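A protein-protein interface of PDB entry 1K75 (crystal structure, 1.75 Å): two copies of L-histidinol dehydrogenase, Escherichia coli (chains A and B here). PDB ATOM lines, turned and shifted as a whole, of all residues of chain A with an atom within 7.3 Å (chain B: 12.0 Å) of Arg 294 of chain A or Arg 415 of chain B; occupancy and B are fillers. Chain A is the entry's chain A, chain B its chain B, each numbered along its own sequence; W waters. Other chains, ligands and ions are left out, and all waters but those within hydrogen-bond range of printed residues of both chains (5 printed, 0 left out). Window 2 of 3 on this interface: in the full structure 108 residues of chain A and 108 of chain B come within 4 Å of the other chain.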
ATOM      1  N   SER A 135      11.022   9.584 -12.093  1.00  0.00           N
ATOM      2  CA  SER A 135      12.429   9.255 -12.301  1.00  0.00           C
ATOM      3  C   SER A 135      13.169   8.936 -11.000  1.00  0.00           C
ATOM      4  O   SER A 135      14.129   8.157 -11.008  1.00  0.00           O
ATOM      5  CB  SER A 135      13.149  10.395 -13.042  1.00  0.00           C
ATOM      6  OG  SER A 135      13.026  11.621 -12.340  1.00  0.00           O
ATOM      7  N   ALA A 136      12.734   9.534  -9.891  1.00  0.00           N
ATOM      8  CA  ALA A 136      13.365   9.280  -8.600  1.00  0.00           C
ATOM      9  C   ALA A 136      12.521   8.273  -7.806  1.00  0.00           C
ATOM     10  O   ALA A 136      11.315   8.445  -7.651  1.00  0.00           O
ATOM     11  CB  ALA A 136      13.507  10.592  -7.818  1.00  0.00           C
ATOM     12  N   PRO A 137      13.145   7.208  -7.287  1.00  0.00           N
ATOM     13  CA  PRO A 137      12.362   6.225  -6.529  1.00  0.00           C
ATOM     14  C   PRO A 137      12.138   6.524  -5.034  1.00  0.00           C
ATOM     15  O   PRO A 137      13.096   6.594  -4.264  1.00  0.00           O
ATOM     16  CB  PRO A 137      13.158   4.938  -6.737  1.00  0.00           C
ATOM     17  CG  PRO A 137      14.574   5.425  -6.703  1.00  0.00           C
ATOM     18  CD  PRO A 137      14.500   6.704  -7.567  1.00  0.00           C
ATOM     19  N   PHE A 139      11.375   4.795  -2.454  1.00  0.00           N
ATOM     20  CA  PHE A 139      11.347   3.527  -1.764  1.00  0.00           C
ATOM     21  C   PHE A 139      11.253   3.638  -0.248  1.00  0.00           C
ATOM     22  O   PHE A 139      10.823   2.703   0.390  1.00  0.00           O
ATOM     23  CB  PHE A 139      12.591   2.719  -2.150  1.00  0.00           C
ATOM     24  CG  PHE A 139      13.881   3.305  -1.626  1.00  0.00           C
ATOM     25  CD1 PHE A 139      14.326   3.020  -0.337  1.00  0.00           C
ATOM     26  CD2 PHE A 139      14.611   4.201  -2.407  1.00  0.00           C
ATOM     27  CE1 PHE A 139      15.472   3.615   0.170  1.00  0.00           C
ATOM     28  CE2 PHE A 139      15.775   4.811  -1.908  1.00  0.00           C
ATOM     29  CZ  PHE A 139      16.201   4.519  -0.626  1.00  0.00           C
ATOM     30  N   GLU A 261      11.659  20.924  -1.334  1.00  0.00           N
ATOM     31  CA  GLU A 261      11.834  20.018  -2.489  1.00  0.00           C
ATOM     32  C   GLU A 261      10.811  18.884  -2.523  1.00  0.00           C
ATOM     33  O   GLU A 261      10.770  18.095  -3.476  1.00  0.00           O
ATOM     34  CB  GLU A 261      13.276  19.449  -2.541  1.00  0.00           C
ATOM     35  CG  GLU A 261      13.611  18.433  -1.418  1.00  0.00           C
ATOM     36  CD  GLU A 261      15.047  17.909  -1.491  1.00  0.00           C
ATOM     37  OE1 GLU A 261      15.790  18.258  -2.434  1.00  0.00           O
ATOM     38  OE2 GLU A 261      15.436  17.124  -0.588  1.00  0.00           O
ATOM     39  N   LEU A 289      20.049  27.112  -2.107  1.00  0.00           N
ATOM     40  CA  LEU A 289      19.195  26.816  -3.261  1.00  0.00           C
ATOM     41  C   LEU A 289      20.024  26.804  -4.552  1.00  0.00           C
ATOM     42  O   LEU A 289      19.796  25.977  -5.442  1.00  0.00           O
ATOM     43  CB  LEU A 289      18.093  27.861  -3.378  1.00  0.00           C
ATOM     44  CG  LEU A 289      17.128  27.786  -4.567  1.00  0.00           C
ATOM     45  CD1 LEU A 289      16.355  26.459  -4.546  1.00  0.00           C
ATOM     46  CD2 LEU A 289      16.171  28.954  -4.504  1.00  0.00           C
ATOM     47  N   GLU A 291      22.890  25.785  -5.027  1.00  0.00           N
ATOM     48  CA  GLU A 291      23.632  24.530  -5.150  1.00  0.00           C
ATOM     49  C   GLU A 291      22.780  23.312  -5.454  1.00  0.00           C
ATOM     50  O   GLU A 291      23.317  22.215  -5.635  1.00  0.00           O
ATOM     51  CB  GLU A 291      24.409  24.242  -3.857  1.00  0.00           C
ATOM     52  CG  GLU A 291      25.317  25.387  -3.486  1.00  0.00           C
ATOM     53  CD  GLU A 291      26.649  24.904  -2.992  1.00  0.00           C
ATOM     54  OE1 GLU A 291      27.180  23.928  -3.561  1.00  0.00           O
ATOM     55  OE2 GLU A 291      27.166  25.496  -2.042  1.00  0.00           O
ATOM     56  N   LEU A 292      21.461  23.481  -5.480  1.00  0.00           N
ATOM     57  CA  LEU A 292      20.576  22.350  -5.749  1.00  0.00           C
ATOM     58  C   LEU A 292      20.365  22.132  -7.239  1.00  0.00           C
ATOM     59  O   LEU A 292      19.893  23.000  -7.941  1.00  0.00           O
ATOM     60  CB  LEU A 292      19.212  22.556  -5.067  1.00  0.00           C
ATOM     61  CG  LEU A 292      19.309  22.610  -3.542  1.00  0.00           C
ATOM     62  CD1 LEU A 292      17.944  22.979  -2.928  1.00  0.00           C
ATOM     63  CD2 LEU A 292      19.743  21.242  -2.987  1.00  0.00           C
ATOM     64  N   PRO A 293      20.674  20.941  -7.723  1.00  0.00           N
ATOM     65  CA  PRO A 293      20.502  20.643  -9.156  1.00  0.00           C
ATOM     66  C   PRO A 293      19.039  20.577  -9.633  1.00  0.00           C
ATOM     67  O   PRO A 293      18.673  21.093 -10.688  1.00  0.00           O
ATOM     68  CB  PRO A 293      21.241  19.317  -9.312  1.00  0.00           C
ATOM     69  CG  PRO A 293      21.028  18.649  -7.945  1.00  0.00           C
ATOM     70  CD  PRO A 293      21.259  19.805  -6.984  1.00  0.00           C
ATOM     71  N   ARG A 294      18.179  19.948  -8.871  1.00  0.00           N
ATOM     72  CA  ARG A 294      16.799  19.859  -9.321  1.00  0.00           C
ATOM     73  C   ARG A 294      16.101  20.815  -8.401  1.00  0.00           C
ATOM     74  O   ARG A 294      15.494  20.404  -7.423  1.00  0.00           O
ATOM     75  CB  ARG A 294      16.313  18.416  -9.153  1.00  0.00           C
ATOM     76  CG  ARG A 294      17.278  17.438  -9.818  1.00  0.00           C
ATOM     77  CD  ARG A 294      17.076  16.012  -9.344  1.00  0.00           C
ATOM     78  NE  ARG A 294      18.162  15.128  -9.769  1.00  0.00           N
ATOM     79  CZ  ARG A 294      19.445  15.283  -9.446  1.00  0.00           C
ATOM     80  NH1 ARG A 294      19.835  16.294  -8.688  1.00  0.00           N
ATOM     81  NH2 ARG A 294      20.350  14.417  -9.881  1.00  0.00           N
ATOM     82  N   ALA A 295      16.186  22.102  -8.700  1.00  0.00           N
ATOM     83  CA  ALA A 295      15.601  23.038  -7.768  1.00  0.00           C
ATOM     84  C   ALA A 295      14.344  23.794  -8.148  1.00  0.00           C
ATOM     85  O   ALA A 295      13.882  24.612  -7.348  1.00  0.00           O
ATOM     86  CB  ALA A 295      16.678  24.030  -7.321  1.00  0.00           C
ATOM     87  N   GLU A 296      13.772  23.552  -9.328  1.00  0.00           N
ATOM     88  CA  GLU A 296      12.562  24.293  -9.674  1.00  0.00           C
ATOM     89  C   GLU A 296      11.421  24.046  -8.684  1.00  0.00           C
ATOM     90  O   GLU A 296      10.718  24.978  -8.302  1.00  0.00           O
ATOM     91  CB  GLU A 296      12.108  23.952 -11.098  1.00  0.00           C
ATOM     92  CG  GLU A 296      13.137  24.372 -12.120  1.00  0.00           C
ATOM     93  CD  GLU A 296      14.002  23.225 -12.622  1.00  0.00           C
ATOM     94  OE1 GLU A 296      14.264  22.263 -11.861  1.00  0.00           O
ATOM     95  OE2 GLU A 296      14.426  23.307 -13.800  1.00  0.00           O
ATOM     96  N   THR A 297      11.226  22.800  -8.272  1.00  0.00           N
ATOM     97  CA  THR A 297      10.157  22.500  -7.319  1.00  0.00           C
ATOM     98  C   THR A 297      10.367  23.332  -6.043  1.00  0.00           C
ATOM     99  O   THR A 297       9.463  24.065  -5.599  1.00  0.00           O
ATOM    100  CB  THR A 297      10.135  20.985  -6.953  1.00  0.00           C
ATOM    101  OG1 THR A 297       9.630  20.234  -8.076  1.00  0.00           O
ATOM    102  CG2 THR A 297       9.218  20.731  -5.703  1.00  0.00           C
ATOM    103  N   ALA A 298      11.558  23.212  -5.465  1.00  0.00           N
ATOM    104  CA  ALA A 298      11.870  23.950  -4.245  1.00  0.00           C
ATOM    105  C   ALA A 298      11.687  25.446  -4.477  1.00  0.00           C
ATOM    106  O   ALA A 298      11.138  26.135  -3.634  1.00  0.00           O
ATOM    107  CB  ALA A 298      13.305  23.664  -3.793  1.00  0.00           C
ATOM    108  N   ARG A 299      12.138  25.951  -5.623  1.00  0.00           N
ATOM    109  CA  ARG A 299      11.992  27.383  -5.903  1.00  0.00           C
ATOM    110  C   ARG A 299      10.532  27.810  -5.848  1.00  0.00           C
ATOM    111  O   ARG A 299      10.191  28.855  -5.282  1.00  0.00           O
ATOM    112  CB  ARG A 299      12.579  27.731  -7.285  1.00  0.00           C
ATOM    113  CG  ARG A 299      12.636  29.244  -7.549  1.00  0.00           C
ATOM    114  CD  ARG A 299      13.323  29.537  -8.882  1.00  0.00           C
ATOM    115  N   TYR A 361      13.921   9.295   6.931  1.00  0.00           N
ATOM    116  CA  TYR A 361      14.601   8.072   6.501  1.00  0.00           C
ATOM    117  C   TYR A 361      14.991   7.015   7.509  1.00  0.00           C
ATOM    118  O   TYR A 361      14.841   5.824   7.228  1.00  0.00           O
ATOM    119  CB  TYR A 361      15.905   8.433   5.755  1.00  0.00           C
ATOM    120  CG  TYR A 361      15.703   9.121   4.424  1.00  0.00           C
ATOM    121  CD1 TYR A 361      15.124   8.430   3.351  1.00  0.00           C
ATOM    122  CD2 TYR A 361      16.042  10.463   4.241  1.00  0.00           C
ATOM    123  CE1 TYR A 361      14.881   9.055   2.133  1.00  0.00           C
ATOM    124  CE2 TYR A 361      15.798  11.107   3.005  1.00  0.00           C
ATOM    125  CZ  TYR A 361      15.214  10.389   1.964  1.00  0.00           C
ATOM    126  OH  TYR A 361      14.932  10.993   0.762  1.00  0.00           O
ATOM    127  N   THR B 406      24.103   6.650   6.845  1.00  0.00           N
ATOM    128  CA  THR B 406      22.899   5.925   6.446  1.00  0.00           C
ATOM    129  C   THR B 406      21.879   6.901   5.824  1.00  0.00           C
ATOM    130  O   THR B 406      21.354   6.633   4.732  1.00  0.00           O
ATOM    131  CB  THR B 406      22.249   5.226   7.661  1.00  0.00           C
ATOM    132  OG1 THR B 406      23.097   4.148   8.095  1.00  0.00           O
ATOM    133  CG2 THR B 406      20.862   4.698   7.306  1.00  0.00           C
ATOM    134  N   ILE B 407      21.607   8.022   6.507  1.00  0.00           N
ATOM    135  CA  ILE B 407      20.645   8.993   5.967  1.00  0.00           C
ATOM    136  C   ILE B 407      21.132   9.549   4.620  1.00  0.00           C
ATOM    137  O   ILE B 407      20.356   9.656   3.669  1.00  0.00           O
ATOM    138  CB  ILE B 407      20.421  10.182   6.934  1.00  0.00           C
ATOM    139  CG1 ILE B 407      19.913   9.668   8.291  1.00  0.00           C
ATOM    140  CG2 ILE B 407      19.395  11.165   6.318  1.00  0.00           C
ATOM    141  CD1 ILE B 407      20.093  10.670   9.423  1.00  0.00           C
ATOM    142  N   GLU B 408      22.421   9.889   4.522  1.00  0.00           N
ATOM    143  CA  GLU B 408      22.938  10.404   3.252  1.00  0.00           C
ATOM    144  C   GLU B 408      22.733   9.378   2.132  1.00  0.00           C
ATOM    145  O   GLU B 408      22.299   9.724   1.059  1.00  0.00           O
ATOM    146  CB  GLU B 408      24.432  10.775   3.358  1.00  0.00           C
ATOM    147  CG  GLU B 408      24.656  12.076   4.136  1.00  0.00           C
ATOM    148  CD  GLU B 408      26.066  12.633   4.032  1.00  0.00           C
ATOM    149  OE1 GLU B 408      26.620  12.702   2.904  1.00  0.00           O
ATOM    150  OE2 GLU B 408      26.612  13.021   5.087  1.00  0.00           O
ATOM    151  N   THR B 409      23.017   8.116   2.411  1.00  0.00           N
ATOM    152  CA  THR B 409      22.859   7.087   1.402  1.00  0.00           C
ATOM    153  C   THR B 409      21.440   7.000   0.889  1.00  0.00           C
ATOM    154  O   THR B 409      21.204   6.967  -0.338  1.00  0.00           O
ATOM    155  CB  THR B 409      23.297   5.725   1.950  1.00  0.00           C
ATOM    156  OG1 THR B 409      24.702   5.785   2.195  1.00  0.00           O
ATOM    157  CG2 THR B 409      23.015   4.590   0.949  1.00  0.00           C
ATOM    158  N   LEU B 410      20.494   6.959   1.821  1.00  0.00           N
ATOM    159  CA  LEU B 410      19.104   6.860   1.451  1.00  0.00           C
ATOM    160  C   LEU B 410      18.614   8.106   0.688  1.00  0.00           C
ATOM    161  O   LEU B 410      17.921   7.969  -0.321  1.00  0.00           O
ATOM    162  CB  LEU B 410      18.247   6.608   2.706  1.00  0.00           C
ATOM    163  CG  LEU B 410      18.568   5.278   3.439  1.00  0.00           C
ATOM    164  CD1 LEU B 410      17.915   5.248   4.817  1.00  0.00           C
ATOM    165  CD2 LEU B 410      18.081   4.104   2.565  1.00  0.00           C
ATOM    166  N   ALA B 411      18.977   9.315   1.141  1.00  0.00           N
ATOM    167  CA  ALA B 411      18.529  10.538   0.463  1.00  0.00           C
ATOM    168  C   ALA B 411      19.089  10.639  -0.954  1.00  0.00           C
ATOM    169  O   ALA B 411      18.405  11.125  -1.875  1.00  0.00           O
ATOM    170  CB  ALA B 411      18.927  11.806   1.277  1.00  0.00           C
ATOM    171  N   ALA B 412      20.324  10.183  -1.125  1.00  0.00           N
ATOM    172  CA  ALA B 412      20.996  10.230  -2.427  1.00  0.00           C
ATOM    173  C   ALA B 412      20.309   9.291  -3.386  1.00  0.00           C
ATOM    174  O   ALA B 412      20.138   9.620  -4.566  1.00  0.00           O
ATOM    175  CB  ALA B 412      22.466   9.823  -2.285  1.00  0.00           C
ATOM    176  N   ALA B 413      19.894   8.139  -2.868  1.00  0.00           N
ATOM    177  CA  ALA B 413      19.217   7.128  -3.680  1.00  0.00           C
ATOM    178  C   ALA B 413      17.846   7.656  -4.112  1.00  0.00           C
ATOM    179  O   ALA B 413      17.382   7.328  -5.186  1.00  0.00           O
ATOM    180  CB  ALA B 413      19.096   5.810  -2.903  1.00  0.00           C
ATOM    181  N   GLU B 414      17.211   8.507  -3.293  1.00  0.00           N
ATOM    182  CA  GLU B 414      15.924   9.083  -3.686  1.00  0.00           C
ATOM    183  C   GLU B 414      16.116  10.374  -4.481  1.00  0.00           C
ATOM    184  O   GLU B 414      15.140  11.008  -4.881  1.00  0.00           O
ATOM    185  CB  GLU B 414      15.028   9.392  -2.463  1.00  0.00           C
ATOM    186  CG  GLU B 414      14.582   8.132  -1.686  1.00  0.00           C
ATOM    187  CD  GLU B 414      13.350   8.382  -0.820  1.00  0.00           C
ATOM    188  OE1 GLU B 414      13.137   9.529  -0.387  1.00  0.00           O
ATOM    189  OE2 GLU B 414      12.592   7.427  -0.550  1.00  0.00           O
ATOM    190  N   ARG B 415      17.373  10.764  -4.670  1.00  0.00           N
ATOM    191  CA  ARG B 415      17.755  11.971  -5.376  1.00  0.00           C
ATOM    192  C   ARG B 415      17.175  13.219  -4.712  1.00  0.00           C
ATOM    193  O   ARG B 415      16.841  14.179  -5.391  1.00  0.00           O
ATOM    194  CB  ARG B 415      17.323  11.913  -6.851  1.00  0.00           C
ATOM    195  CG  ARG B 415      17.763  10.624  -7.550  1.00  0.00           C
ATOM    196  CD  ARG B 415      17.566  10.740  -9.058  1.00  0.00           C
ATOM    197  NE  ARG B 415      18.813  10.517  -9.778  1.00  0.00           N
ATOM    198  CZ  ARG B 415      19.951  11.177  -9.557  1.00  0.00           C
ATOM    199  NH1 ARG B 415      20.018  12.124  -8.630  1.00  0.00           N
ATOM    200  NH2 ARG B 415      21.031  10.876 -10.266  1.00  0.00           N
ATOM    201  N   LEU B 416      17.037  13.186  -3.387  1.00  0.00           N
ATOM    202  CA  LEU B 416      16.524  14.350  -2.656  1.00  0.00           C
ATOM    203  C   LEU B 416      17.741  15.053  -2.089  1.00  0.00           C
ATOM    204  O   LEU B 416      18.145  14.840  -0.941  1.00  0.00           O
ATOM    205  CB  LEU B 416      15.546  13.905  -1.555  1.00  0.00           C
ATOM    206  CG  LEU B 416      14.204  13.465  -2.186  1.00  0.00           C
ATOM    207  CD1 LEU B 416      13.270  12.945  -1.110  1.00  0.00           C
ATOM    208  CD2 LEU B 416      13.580  14.657  -2.929  1.00  0.00           C
ATOM    209  N   THR B 417      18.320  15.903  -2.933  1.00  0.00           N
ATOM    210  CA  THR B 417      19.542  16.615  -2.622  1.00  0.00           C
ATOM    211  C   THR B 417      19.509  17.472  -1.371  1.00  0.00           C
ATOM    212  O   THR B 417      20.469  17.467  -0.599  1.00  0.00           O
ATOM    213  CB  THR B 417      19.986  17.470  -3.843  1.00  0.00           C
ATOM    214  OG1 THR B 417      20.028  16.617  -5.015  1.00  0.00           O
ATOM    215  CG2 THR B 417      21.404  18.056  -3.607  1.00  0.00           C
ATOM    216  N   ALA B 418      18.426  18.212  -1.160  1.00  0.00           N
ATOM    217  CA  ALA B 418      18.367  19.058   0.040  1.00  0.00           C
ATOM    218  C   ALA B 418      18.365  18.185   1.302  1.00  0.00           C
ATOM    219  O   ALA B 418      19.052  18.509   2.294  1.00  0.00           O
ATOM    220  CB  ALA B 418      17.128  19.972  -0.004  1.00  0.00           C
ATOM    221  N   HIS B 419      17.621  17.073   1.268  1.00  0.00           N
ATOM    222  CA  HIS B 419      17.577  16.145   2.406  1.00  0.00           C
ATOM    223  C   HIS B 419      18.991  15.668   2.740  1.00  0.00           C
ATOM    224  O   HIS B 419      19.361  15.516   3.907  1.00  0.00           O
ATOM    225  CB  HIS B 419      16.710  14.900   2.104  1.00  0.00           C
ATOM    226  CG  HIS B 419      15.239  15.110   2.341  1.00  0.00           C
ATOM    227  ND1 HIS B 419      14.485  15.989   1.596  1.00  0.00           N
ATOM    228  CD2 HIS B 419      14.385  14.546   3.234  1.00  0.00           C
ATOM    229  CE1 HIS B 419      13.229  15.962   2.017  1.00  0.00           C
ATOM    230  NE2 HIS B 419      13.141  15.093   3.011  1.00  0.00           N
ATOM    231  N   LYS B 420      19.773  15.420   1.699  1.00  0.00           N
ATOM    232  CA  LYS B 420      21.126  14.961   1.885  1.00  0.00           C
ATOM    233  C   LYS B 420      22.014  16.107   2.374  1.00  0.00           C
ATOM    234  O   LYS B 420      22.839  15.913   3.277  1.00  0.00           O
ATOM    235  CB  LYS B 420      21.693  14.398   0.581  1.00  0.00           C
ATOM    236  CG  LYS B 420      23.142  13.852   0.702  1.00  0.00           C
ATOM    237  CD  LYS B 420      23.706  13.493  -0.692  1.00  0.00           C
ATOM    238  CE  LYS B 420      25.144  12.984  -0.605  1.00  0.00           C
ATOM    239  NZ  LYS B 420      25.581  12.264  -1.850  1.00  0.00           N
ATOM    240  N   ASN B 421      21.832  17.296   1.814  1.00  0.00           N
ATOM    241  CA  ASN B 421      22.695  18.397   2.225  1.00  0.00           C
ATOM    242  C   ASN B 421      22.459  18.791   3.676  1.00  0.00           C
ATOM    243  O   ASN B 421      23.402  19.263   4.339  1.00  0.00           O
ATOM    244  CB  ASN B 421      22.561  19.597   1.279  1.00  0.00           C
ATOM    245  CG  ASN B 421      23.104  19.305  -0.126  1.00  0.00           C
ATOM    246  OD1 ASN B 421      23.794  18.302  -0.362  1.00  0.00           O
ATOM    247  ND2 ASN B 421      22.789  20.185  -1.069  1.00  0.00           N
ATOM    248  N   ALA B 422      21.233  18.560   4.181  1.00  0.00           N
ATOM    249  CA  ALA B 422      20.912  18.869   5.576  1.00  0.00           C
ATOM    250  C   ALA B 422      21.803  18.046   6.477  1.00  0.00           C
ATOM    251  O   ALA B 422      22.222  18.509   7.551  1.00  0.00           O
ATOM    252  CB  ALA B 422      19.434  18.580   5.885  1.00  0.00           C
HETATM  253  O   HOH W   1      24.161  20.302  -3.710  1.00  0.00           O
HETATM  254  O   HOH W   2      21.565  14.502  -7.527  1.00  0.00           O
HETATM  255  O   HOH W   3      16.410  17.427  -4.769  1.00  0.00           O
HETATM  256  O   HOH W   4      18.156  16.168  -6.781  1.00  0.00           O
HETATM  257  O   HOH W   5      18.210  19.310  -6.186  1.00  0.00           O
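Ser 135 of chain A touches none of the printed residues of chain B. Of chain B, only Glu 414 comes within 4 Å of Ala 136 of chain A. Pro 137 of chain A touches just these residues of chain B: Ala 413 and Glu 414. Glu 261 of chain A touches four residues of chain B. Of chain B, only Thr 417 (3.6 Å), Ala 418 (3.8 Å) and Asn 421 (3.8 Å) come within 4 Å of Leu 292 of chain A. Of chain B, only Thr 417 comes within 4 Å of Pro 293 of chain A. Arg 294 of chain A touches two residues of chain B. No residue of chain B comes within 4 Å of Ala 295 of chain A. No residue of chain B comes within 4 Å of Glu 296 of chain A. No residue of chain B comes within 4 Å of Thr 297 of chain A. Ala 298 of chain A touches none of the printed residues of chain B. Of the printed residues of chain A, Ala 411 of chain B touches Tyr 361 (3.6 Å). Arg 415 of chain B touches just one residue of chain A: Arg 294 (2.6 Å). Printed residues of chain A within 4 Å of Ala 418 of chain B: Glu 261 (2.9 Å) and Leu 292 (3.8 Å). Of the printed residues of chain A, His 419 of chain B touches Glu 261 and Tyr 361. Printed residues of chain A within 4 Å of Asn 421 of chain B: Leu 292.
The side-chain carboxylate (OE2) of Glu 414 of chain B lies within hydrogen-bond range of the backbone NH (N) of Phe 139 of chain A, at 3.5 Å. The backbone NH (N) of Thr 417 of chain B is in hydrogen-bond range of the side-chain carboxylate (OE1) of Glu 261 of chain A. OE1 of Glu 261 of chain A lies within hydrogen-bond range of N of Ala 418 of chain B (2.9 Å). The side-chain carboxylate (OE2) of Glu 261 of chain A sits at hydrogen-bond distance from a ring nitrogen (ND1) of His 419 of chain B, 2.6 Å away. NH2 of Arg 294 of chain A sits close to NH1 of Arg 415 of chain B (2.6 Å). The side-chain hydroxyl (OH) of Tyr 361 of chain A sits at hydrogen-bond distance from the side-chain carboxylate (OE1) of Glu 414 of chain B, at 2.6 Å.
No position is printed for both chains.
Printed residues of chain B that touch a printed residue of chain A: Leu 410, Ala 411, Ala 413, Glu 414, Arg 415, Leu 416, Thr 417, Ala 418, His 419 and Asn 421. Hydrophobic or aromatic side chains of chain B that line the printed part of chain A: Leu 410, Ala 411, Ala 413, Leu 416, Ala 418 and His 419. Hydrophobic or aromatic side chains of chain A within 4 Å of the printed part of chain B: Ala 136, Pro 137, Phe 139, Leu 292, Pro 293 and Tyr 361. Among the printed residues, 21 pairs touch across the chains.
Water W4 lies within hydrogen-bond range of the guanidinium group (NH1) of Arg 294 of chain A (2.5 Å), the side-chain hydroxyl (OG1) of Thr 417 of chain B (2.6 Å) and the backbone carbonyl oxygen (O) of Arg 415 of chain B (2.8 Å). Water W3 lies within hydrogen-bond range of OE1 of Glu 261 of chain A, N of Thr 417 of chain B and O of Arg 415 of chain B. Water W2 bridges the guanidinium group (NH2) of Arg 294 of chain A and the guanidinium group (NH1) of Arg 415 of chain B. Water W5 bridges N of Arg 294 of chain A (2.8 Å) and OG1 of Thr 417 of chain B (3.5 Å). Water W1 lies within hydrogen-bond range of the backbone carbonyl oxygen of Glu 291 of chain A (2.8 Å) and the side-chain amide nitrogen of Asn 421 of chain B (3.0 Å).
The backbone carbonyl oxygen (O) of Ala 411 of chain B lies within hydrogen-bond range of the backbone NH (N) of Leu 416 of chain B, 2.9 Å away. O of Thr 417 of chain B lies close to OD1 of Asn 421 of chain B (3.4 Å).
Among the printed residues, pairs that only touch across the chains: Ala 136 of chain A with Glu 414 of chain B, Pro 137 of chain A with Ala 413 of chain B, Pro 137 of chain A with Glu 414 of chain B, Phe 139 of chain A with Leu 410 of chain B, Phe 139 of chain A with Ala 413 of chain B, Glu 261 of chain A with Leu 416 of chain B, Leu 292 of chain A with Thr 417 of chain B, Leu 292 of chain A with Ala 418 of chain B, Leu 292 of chain A with Asn 421 of chain B, Pro 293 of chain A with Thr 417 of chain B, Arg 294 of chain A with Thr 417 of chain B, Tyr 361 of chain A with Leu 410 of chain B, Tyr 361 of chain A with Ala 411 of chain B, Tyr 361 of chain A with Leu 416 of chain B and Tyr 361 of chain A with His 419 of chain B.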
